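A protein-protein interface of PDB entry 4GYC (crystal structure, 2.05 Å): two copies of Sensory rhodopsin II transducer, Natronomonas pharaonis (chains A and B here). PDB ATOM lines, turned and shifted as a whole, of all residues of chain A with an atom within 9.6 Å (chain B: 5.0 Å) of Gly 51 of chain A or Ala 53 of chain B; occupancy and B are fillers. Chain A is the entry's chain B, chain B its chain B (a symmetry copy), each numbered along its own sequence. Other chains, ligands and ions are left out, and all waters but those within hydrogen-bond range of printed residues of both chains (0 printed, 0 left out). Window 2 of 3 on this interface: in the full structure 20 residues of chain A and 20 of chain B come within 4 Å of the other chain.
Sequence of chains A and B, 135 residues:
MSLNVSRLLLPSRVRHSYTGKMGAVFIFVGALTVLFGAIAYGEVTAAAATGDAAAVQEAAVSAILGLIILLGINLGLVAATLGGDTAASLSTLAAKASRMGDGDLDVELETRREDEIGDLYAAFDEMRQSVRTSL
Of chain B, only Ala 53 (3.7 Å) comes within 4 Å of Gly 51 of chain A.
Of chain A, only Gly 51 (3.7 Å) comes within 4 Å of Ala 53 of chain B.
Of chain A, only Ala 53 (3.7 Å) comes within 4 Å of Gly 51 of chain B.
No residue of chain A comes within 4 Å of Asp 52 of chain B.
No residue of chain A comes within 4 Å of Ala 54 of chain B.
Of the printed residues of chain A, Val 56 of chain B touches Val 56 and Gln 57.
Of the printed residues of chain B, Val 56 of chain A touches Val 56 (3.7 Å) and Gln 57 (3.7 Å).
Printed residues of chain A within 4 Å of Gln 57 of chain B: Val 44, Thr 45, Ala 48 and Val 56.
Asp 52 of chain A touches none of the printed residues of chain B.
The nearest residue of chain A that does not touch Ala 53 of chain B is Val 56 of chain A (4.1 Å).
Among the printed residues, pairs that only touch across the chains: Val 44 of chain A with Gln 57 of chain B (3.9 Å), Thr 45 of chain A with Gln 57 of chain B (3.7 Å), Ala 48 of chain A with Gln 57 of chain B (3.1 Å), Gly 51 of chain A with Ala 53 of chain B (3.7 Å), Ala 53 of chain A with Gly 51 of chain B (3.7 Å), Val 56 of chain A with Val 56 of chain B (3.7 Å), Val 56 of chain A with Gln 57 of chain B (3.7 Å) and Gln 57 of chain A with Val 56 of chain B (3.7 Å).
Of the 7 printed residues of chain B, 4 touch a printed residue of chain A.
Of the 15 printed residues of chain A, 7 touch a printed residue of chain B.
Hydrophobic or aromatic side chains of chain A that line the printed part of chain B: Val 44, Ala 48, Ala 53 and Val 56.
Among the printed residues, 8 pairs touch across the chains.
Among the printed residues, no Asp or Glu carboxylate lies within 4 Å of a Lys or Arg side-chain nitrogen of the other chain.
Gly 51 of chain A touches Ala 53 of chain B, and with the chains exchanged Ala 53 of chain A touches Gly 51 of chain B.
Val 56 of chain B touches its own counterpart, Val 56 of chain A.
Val 56 of chain A touches Gln 57 of chain B, and with the chains exchanged Gln 57 of chain A touches Val 56 of chain B.
7 positions are printed for both chains.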
ATOM      1  N   VAL A  44     -14.721   9.822  18.423  1.00  0.00           N
ATOM      2  CA  VAL A  44     -14.101  10.534  19.546  1.00  0.00           C
ATOM      3  C   VAL A  44     -14.514  12.006  19.601  1.00  0.00           C
ATOM      4  O   VAL A  44     -14.831  12.530  20.674  1.00  0.00           O
ATOM      5  CB  VAL A  44     -12.560  10.439  19.501  1.00  0.00           C
ATOM      6  CG1 VAL A  44     -11.937  11.429  20.477  1.00  0.00           C
ATOM      7  CG2 VAL A  44     -12.113   9.025  19.802  1.00  0.00           C
ATOM      8  N   THR A  45     -14.497  12.675  18.452  1.00  0.00           N
ATOM      9  CA  THR A  45     -14.858  14.092  18.403  1.00  0.00           C
ATOM     10  C   THR A  45     -16.351  14.271  18.646  1.00  0.00           C
ATOM     11  O   THR A  45     -16.769  15.231  19.289  1.00  0.00           O
ATOM     12  CB  THR A  45     -14.474  14.738  17.059  1.00  0.00           C
ATOM     13  OG1 THR A  45     -15.285  14.190  16.015  1.00  0.00           O
ATOM     14  CG2 THR A  45     -13.009  14.478  16.745  1.00  0.00           C
ATOM     15  N   ALA A  46     -17.155  13.338  18.144  1.00  0.00           N
ATOM     16  CA  ALA A  46     -18.594  13.388  18.391  1.00  0.00           C
ATOM     17  C   ALA A  46     -18.861  13.251  19.885  1.00  0.00           C
ATOM     18  O   ALA A  46     -19.582  14.054  20.468  1.00  0.00           O
ATOM     19  CB  ALA A  46     -19.327  12.300  17.610  1.00  0.00           C
ATOM     20  N   ALA A  47     -18.267  12.239  20.507  1.00  0.00           N
ATOM     21  CA  ALA A  47     -18.395  12.066  21.951  1.00  0.00           C
ATOM     22  C   ALA A  47     -17.896  13.307  22.703  1.00  0.00           C
ATOM     23  O   ALA A  47     -18.448  13.682  23.743  1.00  0.00           O
ATOM     24  CB  ALA A  47     -17.645  10.813  22.406  1.00  0.00           C
ATOM     25  N   ALA A  48     -16.860  13.940  22.161  1.00  0.00           N
ATOM     26  CA  ALA A  48     -16.253  15.112  22.774  1.00  0.00           C
ATOM     27  C   ALA A  48     -17.243  16.265  22.807  1.00  0.00           C
ATOM     28  O   ALA A  48     -17.302  17.028  23.765  1.00  0.00           O
ATOM     29  CB  ALA A  48     -15.006  15.519  22.006  1.00  0.00           C
ATOM     30  N   ALA A  49     -18.029  16.374  21.745  1.00  0.00           N
ATOM     31  CA  ALA A  49     -18.950  17.482  21.580  1.00  0.00           C
ATOM     32  C   ALA A  49     -20.004  17.525  22.683  1.00  0.00           C
ATOM     33  O   ALA A  49     -20.746  18.498  22.792  1.00  0.00           O
ATOM     34  CB  ALA A  49     -19.608  17.403  20.215  1.00  0.00           C
ATOM     35  N   THR A  50     -20.064  16.479  23.503  1.00  0.00           N
ATOM     36  CA  THR A  50     -21.092  16.388  24.539  1.00  0.00           C
ATOM     37  C   THR A  50     -20.628  16.900  25.903  1.00  0.00           C
ATOM     38  O   THR A  50     -21.450  17.305  26.724  1.00  0.00           O
ATOM     39  CB  THR A  50     -21.623  14.944  24.711  1.00  0.00           C
ATOM     40  OG1 THR A  50     -20.602  14.117  25.280  1.00  0.00           O
ATOM     41  CG2 THR A  50     -22.069  14.359  23.378  1.00  0.00           C
ATOM     42  N   GLY A  51     -19.320  16.880  26.143  1.00  0.00           N
ATOM     43  CA  GLY A  51     -18.776  17.286  27.432  1.00  0.00           C
ATOM     44  C   GLY A  51     -18.763  16.129  28.418  1.00  0.00           C
ATOM     45  O   GLY A  51     -18.293  16.256  29.554  1.00  0.00           O
ATOM     46  N   ASP A  52     -19.276  14.990  27.968  1.00  0.00           N
ATOM     47  CA  ASP A  52     -19.289  13.767  28.760  1.00  0.00           C
ATOM     48  C   ASP A  52     -17.953  13.009  28.600  1.00  0.00           C
ATOM     49  O   ASP A  52     -17.729  12.311  27.606  1.00  0.00           O
ATOM     50  CB  ASP A  52     -20.476  12.893  28.330  1.00  0.00           C
ATOM     51  CG  ASP A  52     -20.683  11.693  29.231  1.00  0.00           C
ATOM     52  OD1 ASP A  52     -19.812  11.424  30.079  1.00  0.00           O
ATOM     53  OD2 ASP A  52     -21.722  11.010  29.081  1.00  0.00           O
ATOM     54  N   ALA A  53     -17.075  13.157  29.588  1.00  0.00           N
ATOM     55  CA  ALA A  53     -15.775  12.496  29.577  1.00  0.00           C
ATOM     56  C   ALA A  53     -15.889  10.989  29.386  1.00  0.00           C
ATOM     57  O   ALA A  53     -15.124  10.393  28.628  1.00  0.00           O
ATOM     58  CB  ALA A  53     -15.015  12.804  30.857  1.00  0.00           C
ATOM     59  N   ALA A  54     -16.839  10.370  30.081  1.00  0.00           N
ATOM     60  CA  ALA A  54     -17.014   8.916  30.010  1.00  0.00           C
ATOM     61  C   ALA A  54     -17.385   8.456  28.599  1.00  0.00           C
ATOM     62  O   ALA A  54     -17.014   7.356  28.168  1.00  0.00           O
ATOM     63  CB  ALA A  54     -18.066   8.451  31.023  1.00  0.00           C
ATOM     64  N   ALA A  55     -18.128   9.305  27.896  1.00  0.00           N
ATOM     65  CA  ALA A  55     -18.556   9.018  26.539  1.00  0.00           C
ATOM     66  C   ALA A  55     -17.361   9.048  25.583  1.00  0.00           C
ATOM     67  O   ALA A  55     -17.262   8.223  24.674  1.00  0.00           O
ATOM     68  CB  ALA A  55     -19.639  10.006  26.096  1.00  0.00           C
ATOM     69  N   VAL A  56     -16.451   9.996  25.791  1.00  0.00           N
ATOM     70  CA  VAL A  56     -15.254  10.055  24.962  1.00  0.00           C
ATOM     71  C   VAL A  56     -14.382   8.838  25.255  1.00  0.00           C
ATOM     72  O   VAL A  56     -13.818   8.229  24.344  1.00  0.00           O
ATOM     73  CB  VAL A  56     -14.435  11.343  25.191  1.00  0.00           C
ATOM     74  CG1 VAL A  56     -13.306  11.426  24.168  1.00  0.00           C
ATOM     75  CG2 VAL A  56     -15.333  12.569  25.097  1.00  0.00           C
ATOM     76  N   GLN A  57     -14.289   8.481  26.532  1.00  0.00           N
ATOM     77  CA  GLN A  57     -13.530   7.312  26.945  1.00  0.00           C
ATOM     78  C   GLN A  57     -14.079   6.061  26.276  1.00  0.00           C
ATOM     79  O   GLN A  57     -13.323   5.219  25.797  1.00  0.00           O
ATOM     80  CB  GLN A  57     -13.565   7.141  28.457  1.00  0.00           C
ATOM     81  CG  GLN A  57     -12.946   5.842  28.928  1.00  0.00           C
ATOM     82  CD  GLN A  57     -12.930   5.712  30.432  1.00  0.00           C
ATOM     83  OE1 GLN A  57     -13.505   6.535  31.141  1.00  0.00           O
ATOM     84  NE2 GLN A  57     -12.273   4.674  30.930  1.00  0.00           N
ATOM     85  N   ALA A  60     -13.092   6.034  22.722  1.00  0.00           N
ATOM     86  CA  ALA A  60     -11.650   5.917  22.590  1.00  0.00           C
ATOM     87  C   ALA A  60     -11.212   4.486  22.853  1.00  0.00           C
ATOM     88  O   ALA A  60     -10.298   3.971  22.205  1.00  0.00           O
ATOM     89  CB  ALA A  60     -10.945   6.898  23.562  1.00  0.00           C
ATOM     90  N   GLY B  51     -12.871  14.365  34.168  1.00  0.00           N
ATOM     91  CA  GLY B  51     -14.175  14.883  33.781  1.00  0.00           C
ATOM     92  C   GLY B  51     -14.059  15.883  32.642  1.00  0.00           C
ATOM     93  O   GLY B  51     -15.060  16.402  32.135  1.00  0.00           O
ATOM     94  N   ASP B  52     -12.822  16.143  32.234  1.00  0.00           N
ATOM     95  CA  ASP B  52     -12.534  17.032  31.116  1.00  0.00           C
ATOM     96  C   ASP B  52     -12.608  16.257  29.782  1.00  0.00           C
ATOM     97  O   ASP B  52     -11.672  15.546  29.403  1.00  0.00           O
ATOM     98  CB  ASP B  52     -11.149  17.665  31.312  1.00  0.00           C
ATOM     99  CG  ASP B  52     -10.847  18.750  30.299  1.00  0.00           C
ATOM    100  OD1 ASP B  52     -11.619  18.898  29.333  1.00  0.00           O
ATOM    101  OD2 ASP B  52      -9.825  19.453  30.468  1.00  0.00           O
ATOM    102  N   ALA B  53     -13.729  16.404  29.082  1.00  0.00           N
ATOM    103  CA  ALA B  53     -13.938  15.741  27.801  1.00  0.00           C
ATOM    104  C   ALA B  53     -12.822  16.031  26.806  1.00  0.00           C
ATOM    105  O   ALA B  53     -12.356  15.132  26.106  1.00  0.00           O
ATOM    106  CB  ALA B  53     -15.281  16.140  27.211  1.00  0.00           C
ATOM    107  N   ALA B  54     -12.399  17.289  26.734  1.00  0.00           N
ATOM    108  CA  ALA B  54     -11.360  17.694  25.782  1.00  0.00           C
ATOM    109  C   ALA B  54     -10.031  16.989  26.058  1.00  0.00           C
ATOM    110  O   ALA B  54      -9.258  16.700  25.134  1.00  0.00           O
ATOM    111  CB  ALA B  54     -11.178  19.216  25.799  1.00  0.00           C
ATOM    112  N   ALA B  55      -9.774  16.730  27.337  1.00  0.00           N
ATOM    113  CA  ALA B  55      -8.557  16.060  27.760  1.00  0.00           C
ATOM    114  C   ALA B  55      -8.570  14.596  27.316  1.00  0.00           C
ATOM    115  O   ALA B  55      -7.546  14.056  26.896  1.00  0.00           O
ATOM    116  CB  ALA B  55      -8.382  16.173  29.277  1.00  0.00           C
ATOM    117  N   VAL B  56      -9.732  13.952  27.407  1.00  0.00           N
ATOM    118  CA  VAL B  56      -9.842  12.574  26.948  1.00  0.00           C
ATOM    119  C   VAL B  56      -9.681  12.537  25.431  1.00  0.00           C
ATOM    120  O   VAL B  56      -9.016  11.653  24.887  1.00  0.00           O
ATOM    121  CB  VAL B  56     -11.186  11.923  27.341  1.00  0.00           C
ATOM    122  CG1 VAL B  56     -11.160  10.437  26.995  1.00  0.00           C
ATOM    123  CG2 VAL B  56     -11.461  12.123  28.824  1.00  0.00           C
ATOM    124  N   GLN B  57     -10.283  13.511  24.757  1.00  0.00           N
ATOM    125  CA  GLN B  57     -10.170  13.621  23.312  1.00  0.00           C
ATOM    126  C   GLN B  57      -8.711  13.768  22.904  1.00  0.00           C
ATOM    127  O   GLN B  57      -8.258  13.140  21.950  1.00  0.00           O
ATOM    128  CB  GLN B  57     -10.969  14.806  22.788  1.00  0.00           C
ATOM    129  CG  GLN B  57     -10.743  15.078  21.316  1.00  0.00           C
ATOM    130  CD  GLN B  57     -11.588  16.214  20.794  1.00  0.00           C
ATOM    131  OE1 GLN B  57     -12.258  16.904  21.559  1.00  0.00           O
ATOM    132  NE2 GLN B  57     -11.560  16.421  19.485  1.00  0.00           N
